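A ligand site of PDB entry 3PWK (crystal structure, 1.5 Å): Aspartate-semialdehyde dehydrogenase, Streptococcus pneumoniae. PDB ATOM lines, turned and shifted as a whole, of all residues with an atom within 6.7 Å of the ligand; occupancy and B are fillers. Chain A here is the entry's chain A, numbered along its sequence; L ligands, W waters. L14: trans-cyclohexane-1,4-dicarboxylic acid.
An oxygen (OAA) of the ligand lies close to the backbone carbonyl oxygen (O) of Gly 159.
Residues that only touch the ligand: Glu 220, Ala 160, Ser 96, Asn 127 and Asn 94.
Hydrophobic or aromatic side chains that line the ligand: Ala 160.
Of the 27 residues printed, 9 come within 4 Å of the ligand.
Along chain A the residues within 4 Å of the ligand span positions 94 to 245.
NZ of Lys 223 is in salt-bridge range of OAB of the ligand, at 2.7 Å.
An oxygen (OAD) of the ligand lies within salt-bridge range of the guanidinium group (NH2) of Arg 99 (2.7 Å).
The guanidinium group of Arg 245 lies within salt-bridge range of an oxygen (OAA) of the ligand, 2.8 Å away.
The side-chain amino group (NZ) of Lys 223 is in salt-bridge range of the side-chain carboxylate (OD2) of Asp 210.
The backbone carbonyl oxygen (O) of Asn 94 lies within hydrogen-bond range of the guanidinium group (NH2) of Arg 99 (2.8 Å).
O of Thr 95 is in hydrogen-bond range of NE of Arg 99.
The side-chain carboxylate (OE2) of Glu 227 lies within salt-bridge range of the guanidinium group (NH1) of Arg 99, 2.9 Å away.
The backbone NH of Gly 159 lies close to the side-chain amide nitrogen of Asn 325 (3.3 Å).
The side-chain amide nitrogen (ND2) of Asn 127 lies within hydrogen-bond range of the side-chain carboxylate (OE1) of Glu 220 (3.3 Å).
OE1 of Glu 227 sits at hydrogen-bond distance from N of Asn 127 (2.9 Å).
The side-chain amide oxygen (OD1) of Asn 94 lies within hydrogen-bond range of the side-chain sulfur (SG) of Cys 125.
Water W2 lies within hydrogen-bond range of OAD of the ligand (2.8 Å) and O of Asn 94 (3.0 Å).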
ATOM      1  N   ASN A  94     -28.745  27.026   5.348  1.00  0.00           N
ATOM      2  CA  ASN A  94     -27.776  26.813   4.268  1.00  0.00           C
ATOM      3  C   ASN A  94     -27.396  28.073   3.511  1.00  0.00           C
ATOM      4  O   ASN A  94     -26.396  28.076   2.776  1.00  0.00           O
ATOM      5  CB  ASN A  94     -28.277  25.788   3.239  1.00  0.00           C
ATOM      6  CG  ASN A  94     -28.032  24.366   3.650  1.00  0.00           C
ATOM      7  OD1 ASN A  94     -26.903  23.855   3.655  1.00  0.00           O
ATOM      8  ND2 ASN A  94     -29.113  23.674   3.931  1.00  0.00           N
ATOM      9  N   THR A  95     -28.150  29.151   3.691  1.00  0.00           N
ATOM     10  CA  THR A  95     -27.905  30.370   2.901  1.00  0.00           C
ATOM     11  C   THR A  95     -26.741  31.183   3.461  1.00  0.00           C
ATOM     12  O   THR A  95     -26.247  30.915   4.558  1.00  0.00           O
ATOM     13  CB  THR A  95     -29.146  31.279   2.801  1.00  0.00           C
ATOM     14  OG1 THR A  95     -29.248  32.103   3.973  1.00  0.00           O
ATOM     15  CG2 THR A  95     -30.434  30.461   2.613  1.00  0.00           C
ATOM     16  N   SER A  96     -26.328  32.191   2.702  1.00  0.00           N
ATOM     17  CA  SER A  96     -25.231  33.051   3.112  1.00  0.00           C
ATOM     18  C   SER A  96     -25.668  34.131   4.108  1.00  0.00           C
ATOM     19  O   SER A  96     -24.825  34.784   4.705  1.00  0.00           O
ATOM     20  CB  SER A  96     -24.601  33.702   1.885  1.00  0.00           C
ATOM     21  OG  SER A  96     -25.545  34.552   1.261  1.00  0.00           O
ATOM     22  N   ARG A  99     -24.275  34.114   7.835  1.00  0.00           N
ATOM     23  CA  ARG A  99     -22.949  33.498   8.048  1.00  0.00           C
ATOM     24  C   ARG A  99     -21.925  34.362   8.779  1.00  0.00           C
ATOM     25  O   ARG A  99     -21.101  33.845   9.531  1.00  0.00           O
ATOM     26  CB  ARG A  99     -22.328  33.028   6.739  1.00  0.00           C
ATOM     27  CG  ARG A  99     -23.074  31.884   6.092  1.00  0.00           C
ATOM     28  CD  ARG A  99     -22.281  31.360   4.908  1.00  0.00           C
ATOM     29  NE  ARG A  99     -23.059  30.350   4.204  1.00  0.00           N
ATOM     30  CZ  ARG A  99     -23.107  30.223   2.880  1.00  0.00           C
ATOM     31  NH1 ARG A  99     -22.351  30.997   2.078  1.00  0.00           N
ATOM     32  NH2 ARG A  99     -23.895  29.304   2.364  1.00  0.00           N
ATOM     33  N   CYS A 125     -24.703  27.046   7.906  1.00  0.00           N
ATOM     34  CA  CYS A 125     -23.878  26.149   7.110  1.00  0.00           C
ATOM     35  C   CYS A 125     -23.034  27.058   6.187  1.00  0.00           C
ATOM     36  O   CYS A 125     -23.584  27.971   5.577  1.00  0.00           O
ATOM     37  CB  CYS A 125     -24.836  25.261   6.307  1.00  0.00           C
ATOM     38  SG  CYS A 125     -24.179  23.908   5.315  1.00  0.00           S
ATOM     39  N   PRO A 126     -21.707  26.804   6.062  1.00  0.00           N
ATOM     40  CA  PRO A 126     -20.902  27.566   5.091  1.00  0.00           C
ATOM     41  C   PRO A 126     -21.239  27.192   3.646  1.00  0.00           C
ATOM     42  O   PRO A 126     -22.034  26.263   3.415  1.00  0.00           O
ATOM     43  CB  PRO A 126     -19.452  27.150   5.412  1.00  0.00           C
ATOM     44  CG  PRO A 126     -19.525  26.429   6.763  1.00  0.00           C
ATOM     45  CD  PRO A 126     -20.891  25.812   6.795  1.00  0.00           C
ATOM     46  N   ASN A 127     -20.671  27.906   2.682  1.00  0.00           N
ATOM     47  CA  ASN A 127     -20.872  27.495   1.289  1.00  0.00           C
ATOM     48  C   ASN A 127     -20.144  26.198   0.991  1.00  0.00           C
ATOM     49  O   ASN A 127     -19.192  25.843   1.706  1.00  0.00           O
ATOM     50  CB  ASN A 127     -20.589  28.613   0.260  1.00  0.00           C
ATOM     51  CG  ASN A 127     -19.138  28.946   0.097  1.00  0.00           C
ATOM     52  OD1 ASN A 127     -18.281  28.419   0.786  1.00  0.00           O
ATOM     53  ND2 ASN A 127     -18.844  29.889  -0.807  1.00  0.00           N
ATOM     54  N   CYS A 128     -20.605  25.456  -0.015  1.00  0.00           N
ATOM     55  CA  CYS A 128     -20.052  24.174  -0.389  1.00  0.00           C
ATOM     56  C   CYS A 128     -18.522  24.218  -0.549  1.00  0.00           C
ATOM     57  O   CYS A 128     -17.759  23.398  -0.006  1.00  0.00           O
ATOM     58  CB  CYS A 128     -20.735  23.738  -1.681  1.00  0.00           C
ATOM     59  SG  CYS A 128     -21.213  25.133  -2.800  1.00  0.00           S
ATOM     60  N   SER A 129     -18.078  25.204  -1.340  1.00  0.00           N
ATOM     61  CA  SER A 129     -16.690  25.277  -1.718  1.00  0.00           C
ATOM     62  C   SER A 129     -15.829  25.417  -0.463  1.00  0.00           C
ATOM     63  O   SER A 129     -14.775  24.804  -0.358  1.00  0.00           O
ATOM     64  CB  SER A 129     -16.464  26.416  -2.700  1.00  0.00           C
ATOM     65  OG  SER A 129     -16.983  27.629  -2.156  1.00  0.00           O
ATOM     66  N   GLN A 155     -16.447  24.112 -10.157  1.00  0.00           N
ATOM     67  CA  GLN A 155     -17.714  23.949  -9.441  1.00  0.00           C
ATOM     68  C   GLN A 155     -18.820  23.444 -10.342  1.00  0.00           C
ATOM     69  O   GLN A 155     -18.986  23.884 -11.491  1.00  0.00           O
ATOM     70  CB  GLN A 155     -18.105  25.235  -8.711  1.00  0.00           C
ATOM     71  CG  GLN A 155     -17.226  25.443  -7.473  1.00  0.00           C
ATOM     72  CD  GLN A 155     -17.466  26.752  -6.733  1.00  0.00           C
ATOM     73  OE1 GLN A 155     -16.567  27.600  -6.674  1.00  0.00           O
ATOM     74  NE2 GLN A 155     -18.652  26.912  -6.149  1.00  0.00           N
ATOM     75  N   ALA A 156     -19.609  22.525  -9.782  1.00  0.00           N
ATOM     76  CA  ALA A 156     -20.752  21.918 -10.451  1.00  0.00           C
ATOM     77  C   ALA A 156     -21.949  22.872 -10.504  1.00  0.00           C
ATOM     78  O   ALA A 156     -22.129  23.709  -9.616  1.00  0.00           O
ATOM     79  CB  ALA A 156     -21.138  20.628  -9.722  1.00  0.00           C
ATOM     80  N   VAL A 157     -22.812  22.696 -11.506  1.00  0.00           N
ATOM     81  CA  VAL A 157     -23.929  23.612 -11.708  1.00  0.00           C
ATOM     82  C   VAL A 157     -25.072  23.427 -10.721  1.00  0.00           C
ATOM     83  O   VAL A 157     -25.860  24.347 -10.525  1.00  0.00           O
ATOM     84  CB  VAL A 157     -24.463  23.563 -13.171  1.00  0.00           C
ATOM     85  CG1 VAL A 157     -23.334  23.988 -14.155  1.00  0.00           C
ATOM     86  CG2 VAL A 157     -24.995  22.165 -13.517  1.00  0.00           C
ATOM     87  N   SER A 158     -25.151  22.262 -10.069  1.00  0.00           N
ATOM     88  CA  SER A 158     -26.294  22.066  -9.148  1.00  0.00           C
ATOM     89  C   SER A 158     -26.192  23.025  -7.969  1.00  0.00           C
ATOM     90  O   SER A 158     -27.184  23.262  -7.291  1.00  0.00           O
ATOM     91  CB  SER A 158     -26.397  20.629  -8.674  1.00  0.00           C
ATOM     92  OG  SER A 158     -25.262  20.255  -7.909  1.00  0.00           O
ATOM     93  N   GLY A 159     -25.000  23.583  -7.729  1.00  0.00           N
ATOM     94  CA  GLY A 159     -24.844  24.596  -6.673  1.00  0.00           C
ATOM     95  C   GLY A 159     -25.697  25.826  -6.922  1.00  0.00           C
ATOM     96  O   GLY A 159     -26.020  26.556  -5.987  1.00  0.00           O
ATOM     97  N   ALA A 160     -26.069  26.067  -8.192  1.00  0.00           N
ATOM     98  CA  ALA A 160     -26.890  27.212  -8.570  1.00  0.00           C
ATOM     99  C   ALA A 160     -28.381  26.881  -8.623  1.00  0.00           C
ATOM    100  O   ALA A 160     -29.193  27.721  -8.990  1.00  0.00           O
ATOM    101  CB  ALA A 160     -26.411  27.770  -9.897  1.00  0.00           C
ATOM    102  N   GLY A 161     -28.750  25.662  -8.237  1.00  0.00           N
ATOM    103  CA  GLY A 161     -30.149  25.272  -8.124  1.00  0.00           C
ATOM    104  C   GLY A 161     -30.631  24.369  -9.237  1.00  0.00           C
ATOM    105  O   GLY A 161     -29.918  24.124 -10.220  1.00  0.00           O
ATOM    106  N   LEU A 190     -27.155  30.854 -15.643  1.00  0.00           N
ATOM    107  CA  LEU A 190     -25.718  30.934 -15.381  1.00  0.00           C
ATOM    108  C   LEU A 190     -25.098  32.127 -16.115  1.00  0.00           C
ATOM    109  O   LEU A 190     -25.601  32.537 -17.150  1.00  0.00           O
ATOM    110  CB  LEU A 190     -25.030  29.625 -15.781  1.00  0.00           C
ATOM    111  CG  LEU A 190     -25.444  28.429 -14.901  1.00  0.00           C
ATOM    112  CD1 LEU A 190     -25.000  27.123 -15.549  1.00  0.00           C
ATOM    113  CD2 LEU A 190     -24.908  28.555 -13.469  1.00  0.00           C
ATOM    114  N   PRO A 191     -24.005  32.686 -15.571  1.00  0.00           N
ATOM    115  CA  PRO A 191     -23.297  32.209 -14.389  1.00  0.00           C
ATOM    116  C   PRO A 191     -24.017  32.512 -13.063  1.00  0.00           C
ATOM    117  O   PRO A 191     -23.827  31.769 -12.093  1.00  0.00           O
ATOM    118  CB  PRO A 191     -21.959  32.967 -14.456  1.00  0.00           C
ATOM    119  CG  PRO A 191     -22.285  34.237 -15.251  1.00  0.00           C
ATOM    120  CD  PRO A 191     -23.234  33.730 -16.287  1.00  0.00           C
ATOM    121  N   ILE A 209     -18.881  33.026 -10.200  1.00  0.00           N
ATOM    122  CA  ILE A 209     -19.913  32.430  -9.357  1.00  0.00           C
ATOM    123  C   ILE A 209     -20.374  33.518  -8.409  1.00  0.00           C
ATOM    124  O   ILE A 209     -19.539  34.196  -7.779  1.00  0.00           O
ATOM    125  CB  ILE A 209     -19.398  31.184  -8.628  1.00  0.00           C
ATOM    126  CG1 ILE A 209     -19.011  30.132  -9.682  1.00  0.00           C
ATOM    127  CG2 ILE A 209     -20.469  30.661  -7.642  1.00  0.00           C
ATOM    128  CD1 ILE A 209     -18.497  28.838  -9.180  1.00  0.00           C
ATOM    129  N   ASP A 210     -21.691  33.696  -8.316  1.00  0.00           N
ATOM    130  CA  ASP A 210     -22.312  34.843  -7.640  1.00  0.00           C
ATOM    131  C   ASP A 210     -21.967  36.131  -8.405  1.00  0.00           C
ATOM    132  O   ASP A 210     -21.450  36.088  -9.524  1.00  0.00           O
ATOM    133  CB  ASP A 210     -21.864  34.896  -6.147  1.00  0.00           C
ATOM    134  CG  ASP A 210     -22.954  35.427  -5.208  1.00  0.00           C
ATOM    135  OD1 ASP A 210     -23.626  36.438  -5.526  1.00  0.00           O
ATOM    136  OD2 ASP A 210     -23.098  34.834  -4.108  1.00  0.00           O
ATOM    137  N   GLU A 220     -18.602  34.701  -4.272  1.00  0.00           N
ATOM    138  CA  GLU A 220     -18.206  33.316  -3.965  1.00  0.00           C
ATOM    139  C   GLU A 220     -16.754  33.275  -3.502  1.00  0.00           C
ATOM    140  O   GLU A 220     -16.439  32.580  -2.525  1.00  0.00           O
ATOM    141  CB  GLU A 220     -18.440  32.402  -5.172  1.00  0.00           C
ATOM    142  CG  GLU A 220     -18.091  30.928  -4.953  1.00  0.00           C
ATOM    143  CD  GLU A 220     -19.156  30.166  -4.213  1.00  0.00           C
ATOM    144  OE1 GLU A 220     -20.079  30.814  -3.683  1.00  0.00           O
ATOM    145  OE2 GLU A 220     -19.062  28.925  -4.162  1.00  0.00           O
ATOM    146  N   LYS A 223     -16.524  34.804  -0.062  1.00  0.00           N
ATOM    147  CA  LYS A 223     -17.076  33.880   0.940  1.00  0.00           C
ATOM    148  C   LYS A 223     -16.035  32.854   1.332  1.00  0.00           C
ATOM    149  O   LYS A 223     -15.862  32.567   2.533  1.00  0.00           O
ATOM    150  CB  LYS A 223     -18.331  33.181   0.418  1.00  0.00           C
ATOM    151  CG  LYS A 223     -19.568  34.037   0.401  1.00  0.00           C
ATOM    152  CD  LYS A 223     -20.654  33.299  -0.337  1.00  0.00           C
ATOM    153  CE  LYS A 223     -21.820  34.225  -0.639  1.00  0.00           C
ATOM    154  NZ  LYS A 223     -22.837  33.568  -1.499  1.00  0.00           N
ATOM    155  N   GLU A 227     -15.287  33.048   5.213  1.00  0.00           N
ATOM    156  CA  GLU A 227     -15.787  31.866   5.919  1.00  0.00           C
ATOM    157  C   GLU A 227     -14.655  31.018   6.471  1.00  0.00           C
ATOM    158  O   GLU A 227     -14.749  30.534   7.604  1.00  0.00           O
ATOM    159  CB  GLU A 227     -16.720  31.054   5.024  1.00  0.00           C
ATOM    160  CG  GLU A 227     -17.984  31.868   4.702  1.00  0.00           C
ATOM    161  CD  GLU A 227     -18.934  31.171   3.757  1.00  0.00           C
ATOM    162  OE1 GLU A 227     -18.870  29.936   3.684  1.00  0.00           O
ATOM    163  OE2 GLU A 227     -19.758  31.831   3.100  1.00  0.00           O
ATOM    164  N   ARG A 245     -17.186  27.953 -12.707  1.00  0.00           N
ATOM    165  CA  ARG A 245     -18.221  26.951 -12.996  1.00  0.00           C
ATOM    166  C   ARG A 245     -17.787  26.168 -14.233  1.00  0.00           C
ATOM    167  O   ARG A 245     -17.343  26.752 -15.245  1.00  0.00           O
ATOM    168  CB  ARG A 245     -19.556  27.630 -13.273  1.00  0.00           C
ATOM    169  CG  ARG A 245     -20.728  26.636 -13.271  1.00  0.00           C
ATOM    170  CD  ARG A 245     -21.170  26.359 -11.823  1.00  0.00           C
ATOM    171  NE  ARG A 245     -21.781  27.548 -11.246  1.00  0.00           N
ATOM    172  CZ  ARG A 245     -22.259  27.619 -10.011  1.00  0.00           C
ATOM    173  NH1 ARG A 245     -22.240  26.543  -9.231  1.00  0.00           N
ATOM    174  NH2 ARG A 245     -22.762  28.766  -9.543  1.00  0.00           N
ATOM    175  N   HIS A 252     -18.132  19.386  -6.503  1.00  0.00           N
ATOM    176  CA  HIS A 252     -17.136  20.421  -6.743  1.00  0.00           C
ATOM    177  C   HIS A 252     -15.753  19.842  -6.583  1.00  0.00           C
ATOM    178  O   HIS A 252     -15.507  19.011  -5.688  1.00  0.00           O
ATOM    179  CB  HIS A 252     -17.239  21.541  -5.699  1.00  0.00           C
ATOM    180  CG  HIS A 252     -18.491  22.360  -5.784  1.00  0.00           C
ATOM    181  ND1 HIS A 252     -19.314  22.387  -6.888  1.00  0.00           N
ATOM    182  CD2 HIS A 252     -19.021  23.255  -4.910  1.00  0.00           C
ATOM    183  CE1 HIS A 252     -20.309  23.238  -6.687  1.00  0.00           C
ATOM    184  NE2 HIS A 252     -20.143  23.781  -5.494  1.00  0.00           N
ATOM    185  N   ASN A 325     -21.441  18.478  -3.773  1.00  0.00           N
ATOM    186  CA  ASN A 325     -21.779  19.817  -3.310  1.00  0.00           C
ATOM    187  C   ASN A 325     -23.164  19.945  -2.700  1.00  0.00           C
ATOM    188  O   ASN A 325     -23.464  20.923  -2.007  1.00  0.00           O
ATOM    189  CB  ASN A 325     -21.633  20.825  -4.461  1.00  0.00           C
ATOM    190  CG  ASN A 325     -22.556  20.514  -5.626  1.00  0.00           C
ATOM    191  OD1 ASN A 325     -22.393  19.492  -6.286  1.00  0.00           O
ATOM    192  ND2 ASN A 325     -23.548  21.361  -5.851  1.00  0.00           N
ATOM    193  N   GLY A 329     -21.485  19.463   0.912  1.00  0.00           N
ATOM    194  CA  GLY A 329     -21.556  20.877   0.584  1.00  0.00           C
ATOM    195  C   GLY A 329     -22.819  21.591   1.012  1.00  0.00           C
ATOM    196  O   GLY A 329     -22.874  22.820   0.998  1.00  0.00           O
HETATM  197  OAA L14 L   1     -24.102  28.899  -7.121  1.00  0.00           O
HETATM  198  OAB L14 L   1     -23.481  31.133  -0.506  1.00  0.00           O
HETATM  199  OAC L14 L   1     -22.862  27.136  -6.583  1.00  0.00           O
HETATM  200  OAD L14 L   1     -24.255  29.069  -0.348  1.00  0.00           O
HETATM  201  CAE L14 L   1     -25.078  29.131  -4.526  1.00  0.00           C
HETATM  202  CAF L14 L   1     -25.167  29.352  -3.019  1.00  0.00           C
HETATM  203  CAG L14 L   1     -22.562  28.957  -4.330  1.00  0.00           C
HETATM  204  CAH L14 L   1     -22.643  29.190  -2.837  1.00  0.00           C
HETATM  205  CAI L14 L   1     -23.591  28.100  -6.290  1.00  0.00           C
HETATM  206  CAJ L14 L   1     -23.879  30.069  -1.006  1.00  0.00           C
HETATM  207  CAK L14 L   1     -23.838  28.291  -4.834  1.00  0.00           C
HETATM  208  CAL L14 L   1     -23.892  29.998  -2.491  1.00  0.00           C
HETATM  209  O   HOH W   1     -25.455  31.177  -7.610  1.00  0.00           O
HETATM  210  O   HOH W   2     -26.959  28.257  -0.132  1.00  0.00           O
